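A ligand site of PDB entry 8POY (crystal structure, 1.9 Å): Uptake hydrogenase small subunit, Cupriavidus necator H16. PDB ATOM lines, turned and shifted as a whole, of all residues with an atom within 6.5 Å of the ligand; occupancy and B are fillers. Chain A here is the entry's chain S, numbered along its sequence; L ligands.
C of Arg 192 touches S2 of the ligand (3.7 Å). Phe 196 touches the ligand (CB to S2, 3.9 Å). Tyr 217 touches the ligand (CB to S3, 3.8 Å). CA of Gly 223 touches S4 of the ligand, at 3.9 Å. Pro 224 touches the ligand. Ile 243 touches the ligand. Hydrophobic or aromatic side chains that line the ligand: His 187, Phe 196, Leu 216, Tyr 217, Pro 224 and Ile 243. The nearest printed residue that does not touch the ligand is Ile 186 (4.3 Å).
FE1 of the ligand is bound by ND1 of His 187, at 2.1 Å. SG of Cys 215 binds FE4 of the ligand (2.3 Å). The side-chain sulfur (SG) of Cys 221 binds an iron atom (FE2) of the ligand, at 2.3 Å. SG of Cys 190 is bound to FE3 of the ligand (2.3 Å). The backbone NH (N) of Leu 216 sits close to a sulfur (S1) of the ligand (3.4 Å). N of Arg 193 sits close to S2 of the ligand.
N of His 187 is in hydrogen-bond range of O of Gly 223, 3.2 Å away. The side-chain sulfur of Cys 215 sits close to the backbone NH of Tyr 217 (3.3 Å). The backbone carbonyl oxygen (O) of Leu 216 is in hydrogen-bond range of the backbone NH (N) of Cys 221 (3.2 Å). The side-chain sulfur of Cys 221 lies close to the backbone NH of Cys 249. N of Arg 192 sits close to SG of Cys 190 (3.4 Å). The backbone carbonyl oxygen (O) of Ile 243 is in hydrogen-bond range of the guanidinium group (NH2) of Arg 192, 3.1 Å away. The backbone carbonyl oxygen (O) of Phe 214 is in hydrogen-bond range of the guanidinium group (NH1) of Arg 192, 2.7 Å away. The backbone carbonyl oxygen (O) of Gly 223 lies within hydrogen-bond range of the backbone NH (N) of Ile 186, at 3.5 Å.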
ATOM      1  N   ILE A 186      15.375  -1.205 -12.663  1.00  0.00           N
ATOM      2  CA  ILE A 186      16.185  -1.977 -11.713  1.00  0.00           C
ATOM      3  C   ILE A 186      17.611  -1.430 -11.650  1.00  0.00           C
ATOM      4  O   ILE A 186      18.186  -1.286 -10.569  1.00  0.00           O
ATOM      5  CB  ILE A 186      16.304  -3.473 -12.096  1.00  0.00           C
ATOM      6  CG1 ILE A 186      14.925  -4.119 -12.355  1.00  0.00           C
ATOM      7  CG2 ILE A 186      17.027  -4.257 -11.002  1.00  0.00           C
ATOM      8  CD1 ILE A 186      13.912  -3.954 -11.247  1.00  0.00           C
ATOM      9  N   HIS A 187      18.157  -1.133 -12.819  1.00  0.00           N
ATOM     10  CA  HIS A 187      19.529  -0.631 -12.981  1.00  0.00           C
ATOM     11  C   HIS A 187      19.834   0.687 -12.242  1.00  0.00           C
ATOM     12  O   HIS A 187      20.986   0.946 -11.886  1.00  0.00           O
ATOM     13  CB  HIS A 187      19.802  -0.489 -14.492  1.00  0.00           C
ATOM     14  CG  HIS A 187      21.210  -0.122 -14.833  1.00  0.00           C
ATOM     15  ND1 HIS A 187      22.190  -1.068 -15.037  1.00  0.00           N
ATOM     16  CD2 HIS A 187      21.790   1.077 -15.076  1.00  0.00           C
ATOM     17  CE1 HIS A 187      23.319  -0.471 -15.357  1.00  0.00           C
ATOM     18  NE2 HIS A 187      23.111   0.826 -15.386  1.00  0.00           N
ATOM     19  N   ASP A 188      18.797   1.511 -12.000  1.00  0.00           N
ATOM     20  CA  ASP A 188      19.000   2.828 -11.367  1.00  0.00           C
ATOM     21  C   ASP A 188      19.686   2.719 -10.008  1.00  0.00           C
ATOM     22  O   ASP A 188      20.664   3.426  -9.765  1.00  0.00           O
ATOM     23  CB  ASP A 188      17.676   3.580 -11.184  1.00  0.00           C
ATOM     24  CG  ASP A 188      17.033   3.999 -12.498  1.00  0.00           C
ATOM     25  OD1 ASP A 188      17.733   4.001 -13.529  1.00  0.00           O
ATOM     26  OD2 ASP A 188      15.828   4.325 -12.486  1.00  0.00           O
ATOM     27  N   CYS A 190      20.455  -0.529  -8.433  1.00  0.00           N
ATOM     28  CA  CYS A 190      21.057  -1.848  -8.243  1.00  0.00           C
ATOM     29  C   CYS A 190      22.402  -1.705  -7.548  1.00  0.00           C
ATOM     30  O   CYS A 190      23.249  -0.932  -7.969  1.00  0.00           O
ATOM     31  CB  CYS A 190      21.245  -2.559  -9.588  1.00  0.00           C
ATOM     32  SG  CYS A 190      22.104  -4.144  -9.469  1.00  0.00           S
ATOM     33  N   TYR A 191      22.590  -2.464  -6.475  1.00  0.00           N
ATOM     34  CA  TYR A 191      23.826  -2.372  -5.679  1.00  0.00           C
ATOM     35  C   TYR A 191      25.089  -2.799  -6.453  1.00  0.00           C
ATOM     36  O   TYR A 191      26.187  -2.525  -6.013  1.00  0.00           O
ATOM     37  CB  TYR A 191      23.699  -3.203  -4.386  1.00  0.00           C
ATOM     38  CG  TYR A 191      23.962  -4.666  -4.599  1.00  0.00           C
ATOM     39  CD1 TYR A 191      22.970  -5.501  -5.115  1.00  0.00           C
ATOM     40  CD2 TYR A 191      25.210  -5.212  -4.298  1.00  0.00           C
ATOM     41  CE1 TYR A 191      23.223  -6.834  -5.333  1.00  0.00           C
ATOM     42  CE2 TYR A 191      25.468  -6.556  -4.508  1.00  0.00           C
ATOM     43  CZ  TYR A 191      24.469  -7.359  -5.023  1.00  0.00           C
ATOM     44  OH  TYR A 191      24.716  -8.687  -5.229  1.00  0.00           O
ATOM     45  N   ARG A 192      24.925  -3.478  -7.598  1.00  0.00           N
ATOM     46  CA  ARG A 192      26.056  -3.800  -8.485  1.00  0.00           C
ATOM     47  C   ARG A 192      26.371  -2.680  -9.496  1.00  0.00           C
ATOM     48  O   ARG A 192      27.283  -2.812 -10.302  1.00  0.00           O
ATOM     49  CB  ARG A 192      25.808  -5.120  -9.214  1.00  0.00           C
ATOM     50  CG  ARG A 192      25.611  -6.314  -8.276  1.00  0.00           C
ATOM     51  CD  ARG A 192      25.697  -7.648  -9.006  1.00  0.00           C
ATOM     52  NE  ARG A 192      25.460  -8.775  -8.092  1.00  0.00           N
ATOM     53  CZ  ARG A 192      25.911 -10.022  -8.283  1.00  0.00           C
ATOM     54  NH1 ARG A 192      26.653 -10.340  -9.348  1.00  0.00           N
ATOM     55  NH2 ARG A 192      25.625 -10.955  -7.388  1.00  0.00           N
ATOM     56  N   ARG A 193      25.633  -1.582  -9.439  1.00  0.00           N
ATOM     57  CA  ARG A 193      25.823  -0.470 -10.367  1.00  0.00           C
ATOM     58  C   ARG A 193      27.259   0.061 -10.396  1.00  0.00           C
ATOM     59  O   ARG A 193      27.792   0.334 -11.469  1.00  0.00           O
ATOM     60  CB  ARG A 193      24.825   0.657 -10.061  1.00  0.00           C
ATOM     61  CG  ARG A 193      24.900   1.865 -10.982  1.00  0.00           C
ATOM     62  CD  ARG A 193      24.566   1.486 -12.408  1.00  0.00           C
ATOM     63  NE  ARG A 193      24.683   2.639 -13.300  1.00  0.00           N
ATOM     64  CZ  ARG A 193      23.739   3.555 -13.507  1.00  0.00           C
ATOM     65  NH1 ARG A 193      22.572   3.474 -12.887  1.00  0.00           N
ATOM     66  NH2 ARG A 193      23.972   4.550 -14.354  1.00  0.00           N
ATOM     67  N   PRO A 194      27.906   0.224  -9.219  1.00  0.00           N
ATOM     68  CA  PRO A 194      29.293   0.679  -9.265  1.00  0.00           C
ATOM     69  C   PRO A 194      30.213  -0.246 -10.073  1.00  0.00           C
ATOM     70  O   PRO A 194      31.145   0.240 -10.714  1.00  0.00           O
ATOM     71  CB  PRO A 194      29.708   0.716  -7.787  1.00  0.00           C
ATOM     72  CG  PRO A 194      28.434   0.952  -7.059  1.00  0.00           C
ATOM     73  CD  PRO A 194      27.398   0.188  -7.838  1.00  0.00           C
ATOM     74  N   HIS A 195      29.943  -1.554 -10.069  1.00  0.00           N
ATOM     75  CA  HIS A 195      30.701  -2.490 -10.909  1.00  0.00           C
ATOM     76  C   HIS A 195      30.429  -2.269 -12.400  1.00  0.00           C
ATOM     77  O   HIS A 195      31.364  -2.262 -13.212  1.00  0.00           O
ATOM     78  CB  HIS A 195      30.423  -3.942 -10.506  1.00  0.00           C
ATOM     79  CG  HIS A 195      30.940  -4.297  -9.145  1.00  0.00           C
ATOM     80  ND1 HIS A 195      32.275  -4.205  -8.812  1.00  0.00           N
ATOM     81  CD2 HIS A 195      30.304  -4.722  -8.032  1.00  0.00           C
ATOM     82  CE1 HIS A 195      32.435  -4.579  -7.556  1.00  0.00           C
ATOM     83  NE2 HIS A 195      31.260  -4.888  -7.062  1.00  0.00           N
ATOM     84  N   PHE A 196      29.153  -2.086 -12.743  1.00  0.00           N
ATOM     85  CA  PHE A 196      28.788  -1.715 -14.113  1.00  0.00           C
ATOM     86  C   PHE A 196      29.542  -0.443 -14.558  1.00  0.00           C
ATOM     87  O   PHE A 196      30.103  -0.404 -15.654  1.00  0.00           O
ATOM     88  CB  PHE A 196      27.274  -1.482 -14.228  1.00  0.00           C
ATOM     89  CG  PHE A 196      26.848  -0.972 -15.576  1.00  0.00           C
ATOM     90  CD1 PHE A 196      26.535  -1.846 -16.596  1.00  0.00           C
ATOM     91  CD2 PHE A 196      26.757   0.403 -15.826  1.00  0.00           C
ATOM     92  CE1 PHE A 196      26.151  -1.375 -17.843  1.00  0.00           C
ATOM     93  CE2 PHE A 196      26.366   0.878 -17.061  1.00  0.00           C
ATOM     94  CZ  PHE A 196      26.062  -0.015 -18.076  1.00  0.00           C
ATOM     95  N   PHE A 201      32.497  -6.976 -14.937  1.00  0.00           N
ATOM     96  CA  PHE A 201      31.411  -7.901 -15.310  1.00  0.00           C
ATOM     97  C   PHE A 201      31.755  -9.352 -15.077  1.00  0.00           C
ATOM     98  O   PHE A 201      32.908  -9.772 -15.223  1.00  0.00           O
ATOM     99  CB  PHE A 201      31.043  -7.736 -16.785  1.00  0.00           C
ATOM    100  CG  PHE A 201      30.720  -6.334 -17.187  1.00  0.00           C
ATOM    101  CD1 PHE A 201      29.499  -5.764 -16.861  1.00  0.00           C
ATOM    102  CD2 PHE A 201      31.636  -5.584 -17.932  1.00  0.00           C
ATOM    103  CE1 PHE A 201      29.200  -4.463 -17.244  1.00  0.00           C
ATOM    104  CE2 PHE A 201      31.336  -4.291 -18.330  1.00  0.00           C
ATOM    105  CZ  PHE A 201      30.117  -3.728 -17.974  1.00  0.00           C
ATOM    106  N   PHE A 214      30.273  -8.972  -9.191  1.00  0.00           N
ATOM    107  CA  PHE A 214      30.365  -8.061 -10.327  1.00  0.00           C
ATOM    108  C   PHE A 214      29.059  -8.003 -11.120  1.00  0.00           C
ATOM    109  O   PHE A 214      28.211  -8.888 -10.996  1.00  0.00           O
ATOM    110  CB  PHE A 214      31.529  -8.486 -11.250  1.00  0.00           C
ATOM    111  CG  PHE A 214      32.908  -8.034 -10.786  1.00  0.00           C
ATOM    112  CD1 PHE A 214      33.135  -7.566  -9.485  1.00  0.00           C
ATOM    113  CD2 PHE A 214      33.989  -8.099 -11.654  1.00  0.00           C
ATOM    114  CE1 PHE A 214      34.405  -7.154  -9.089  1.00  0.00           C
ATOM    115  CE2 PHE A 214      35.264  -7.695 -11.261  1.00  0.00           C
ATOM    116  CZ  PHE A 214      35.463  -7.229  -9.977  1.00  0.00           C
ATOM    117  N   CYS A 215      28.928  -6.959 -11.937  1.00  0.00           N
ATOM    118  CA  CYS A 215      27.706  -6.718 -12.706  1.00  0.00           C
ATOM    119  C   CYS A 215      27.373  -7.890 -13.631  1.00  0.00           C
ATOM    120  O   CYS A 215      28.271  -8.549 -14.171  1.00  0.00           O
ATOM    121  CB  CYS A 215      27.851  -5.442 -13.532  1.00  0.00           C
ATOM    122  SG  CYS A 215      26.501  -5.159 -14.701  1.00  0.00           S
ATOM    123  N   LEU A 216      26.075  -8.125 -13.808  1.00  0.00           N
ATOM    124  CA  LEU A 216      25.579  -9.280 -14.559  1.00  0.00           C
ATOM    125  C   LEU A 216      25.115  -8.935 -15.980  1.00  0.00           C
ATOM    126  O   LEU A 216      24.509  -9.767 -16.654  1.00  0.00           O
ATOM    127  CB  LEU A 216      24.438  -9.962 -13.794  1.00  0.00           C
ATOM    128  CG  LEU A 216      24.861 -10.600 -12.477  1.00  0.00           C
ATOM    129  CD1 LEU A 216      23.636 -10.884 -11.622  1.00  0.00           C
ATOM    130  CD2 LEU A 216      25.671 -11.860 -12.707  1.00  0.00           C
ATOM    131  N   TYR A 217      25.428  -7.726 -16.442  1.00  0.00           N
ATOM    132  CA  TYR A 217      25.011  -7.265 -17.775  1.00  0.00           C
ATOM    133  C   TYR A 217      25.418  -8.244 -18.883  1.00  0.00           C
ATOM    134  O   TYR A 217      24.606  -8.600 -19.719  1.00  0.00           O
ATOM    135  CB  TYR A 217      25.604  -5.891 -18.044  1.00  0.00           C
ATOM    136  CG  TYR A 217      25.184  -5.240 -19.355  1.00  0.00           C
ATOM    137  CD1 TYR A 217      24.045  -4.443 -19.426  1.00  0.00           C
ATOM    138  CD2 TYR A 217      25.962  -5.389 -20.499  1.00  0.00           C
ATOM    139  CE1 TYR A 217      23.680  -3.829 -20.612  1.00  0.00           C
ATOM    140  CE2 TYR A 217      25.598  -4.772 -21.693  1.00  0.00           C
ATOM    141  CZ  TYR A 217      24.467  -3.998 -21.750  1.00  0.00           C
ATOM    142  OH  TYR A 217      24.091  -3.392 -22.930  1.00  0.00           O
ATOM    143  N   LYS A 218      26.662  -8.714 -18.857  1.00  0.00           N
ATOM    144  CA  LYS A 218      27.160  -9.611 -19.915  1.00  0.00           C
ATOM    145  C   LYS A 218      26.600 -11.044 -19.796  1.00  0.00           C
ATOM    146  O   LYS A 218      26.737 -11.831 -20.733  1.00  0.00           O
ATOM    147  CB  LYS A 218      28.683  -9.610 -19.956  1.00  0.00           C
ATOM    148  CG  LYS A 218      29.281  -8.255 -20.275  1.00  0.00           C
ATOM    149  CD  LYS A 218      30.788  -8.303 -20.481  1.00  0.00           C
ATOM    150  CE  LYS A 218      31.288  -7.020 -21.120  1.00  0.00           C
ATOM    151  NZ  LYS A 218      32.778  -6.956 -21.196  1.00  0.00           N
ATOM    152  N   CYS A 221      21.629  -9.665 -18.031  1.00  0.00           N
ATOM    153  CA  CYS A 221      20.783  -8.924 -17.099  1.00  0.00           C
ATOM    154  C   CYS A 221      20.013  -7.833 -17.826  1.00  0.00           C
ATOM    155  O   CYS A 221      20.606  -7.007 -18.501  1.00  0.00           O
ATOM    156  CB  CYS A 221      21.608  -8.300 -15.966  1.00  0.00           C
ATOM    157  SG  CYS A 221      20.564  -7.404 -14.777  1.00  0.00           S
ATOM    158  N   LYS A 222      18.696  -7.831 -17.670  1.00  0.00           N
ATOM    159  CA  LYS A 222      17.813  -6.901 -18.352  1.00  0.00           C
ATOM    160  C   LYS A 222      17.362  -5.780 -17.414  1.00  0.00           C
ATOM    161  O   LYS A 222      16.405  -5.045 -17.706  1.00  0.00           O
ATOM    162  CB  LYS A 222      16.605  -7.646 -18.903  1.00  0.00           C
ATOM    163  CG  LYS A 222      16.939  -8.753 -19.901  1.00  0.00           C
ATOM    164  CD  LYS A 222      17.876  -8.269 -21.001  1.00  0.00           C
ATOM    165  CE  LYS A 222      17.929  -9.242 -22.170  1.00  0.00           C
ATOM    166  NZ  LYS A 222      18.523 -10.573 -21.822  1.00  0.00           N
ATOM    167  N   GLY A 223      18.062  -5.626 -16.296  1.00  0.00           N
ATOM    168  CA  GLY A 223      17.815  -4.512 -15.379  1.00  0.00           C
ATOM    169  C   GLY A 223      17.794  -3.112 -15.988  1.00  0.00           C
ATOM    170  O   GLY A 223      17.019  -2.270 -15.549  1.00  0.00           O
ATOM    171  N   PRO A 224      18.659  -2.847 -17.004  1.00  0.00           N
ATOM    172  CA  PRO A 224      18.661  -1.539 -17.668  1.00  0.00           C
ATOM    173  C   PRO A 224      17.415  -1.186 -18.495  1.00  0.00           C
ATOM    174  O   PRO A 224      17.245  -0.027 -18.857  1.00  0.00           O
ATOM    175  CB  PRO A 224      19.886  -1.597 -18.574  1.00  0.00           C
ATOM    176  CG  PRO A 224      20.802  -2.572 -17.915  1.00  0.00           C
ATOM    177  CD  PRO A 224      19.881  -3.609 -17.341  1.00  0.00           C
ATOM    178  N   PHE A 241      17.121 -10.221  -4.019  1.00  0.00           N
ATOM    179  CA  PHE A 241      16.435 -10.096  -5.306  1.00  0.00           C
ATOM    180  C   PHE A 241      17.282 -10.787  -6.371  1.00  0.00           C
ATOM    181  O   PHE A 241      18.424 -11.161  -6.096  1.00  0.00           O
ATOM    182  CB  PHE A 241      16.068  -8.622  -5.632  1.00  0.00           C
ATOM    183  CG  PHE A 241      17.224  -7.759  -6.048  1.00  0.00           C
ATOM    184  CD1 PHE A 241      18.220  -7.411  -5.148  1.00  0.00           C
ATOM    185  CD2 PHE A 241      17.259  -7.212  -7.330  1.00  0.00           C
ATOM    186  CE1 PHE A 241      19.257  -6.574  -5.531  1.00  0.00           C
ATOM    187  CE2 PHE A 241      18.288  -6.380  -7.715  1.00  0.00           C
ATOM    188  CZ  PHE A 241      19.298  -6.060  -6.814  1.00  0.00           C
ATOM    189  N   ILE A 243      19.231 -10.316  -8.813  1.00  0.00           N
ATOM    190  CA  ILE A 243      20.616  -9.881  -9.010  1.00  0.00           C
ATOM    191  C   ILE A 243      21.476 -10.138  -7.766  1.00  0.00           C
ATOM    192  O   ILE A 243      22.623 -10.577  -7.899  1.00  0.00           O
ATOM    193  CB  ILE A 243      20.657  -8.392  -9.441  1.00  0.00           C
ATOM    194  CG1 ILE A 243      20.114  -8.266 -10.877  1.00  0.00           C
ATOM    195  CG2 ILE A 243      22.068  -7.806  -9.333  1.00  0.00           C
ATOM    196  CD1 ILE A 243      19.532  -6.909 -11.201  1.00  0.00           C
ATOM    197  N   GLY A 248      20.937 -12.634 -13.416  1.00  0.00           N
ATOM    198  CA  GLY A 248      20.509 -11.374 -13.992  1.00  0.00           C
ATOM    199  C   GLY A 248      18.994 -11.261 -14.035  1.00  0.00           C
ATOM    200  O   GLY A 248      18.273 -12.265 -14.066  1.00  0.00           O
ATOM    201  N   CYS A 249      18.506 -10.030 -13.999  1.00  0.00           N
ATOM    202  CA  CYS A 249      17.111  -9.777 -14.259  1.00  0.00           C
ATOM    203  C   CYS A 249      16.788 -10.345 -15.639  1.00  0.00           C
ATOM    204  O   CYS A 249      17.556 -10.149 -16.591  1.00  0.00           O
ATOM    205  CB  CYS A 249      16.827  -8.269 -14.206  1.00  0.00           C
ATOM    206  SG  CYS A 249      15.153  -7.797 -14.669  1.00  0.00           S
HETATM  207 FE1  LIG L   1      22.444  -2.898 -14.066  1.00  0.00          FE
HETATM  208 FE2  LIG L   1      21.936  -5.735 -13.988  1.00  0.00          FE
HETATM  209 FE3  LIG L   1      22.655  -4.393 -11.689  1.00  0.00          FE
HETATM  210 FE4  LIG L   1      24.501  -4.777 -13.652  1.00  0.00          FE
HETATM  211  S1  LIG L   1      23.498  -6.420 -12.473  1.00  0.00           S
HETATM  212  S2  LIG L   1      24.131  -2.872 -12.471  1.00  0.00           S
HETATM  213  S3  LIG L   1      23.112  -4.524 -15.496  1.00  0.00           S
HETATM  214  S4  LIG L   1      20.796  -4.041 -12.977  1.00  0.00           S
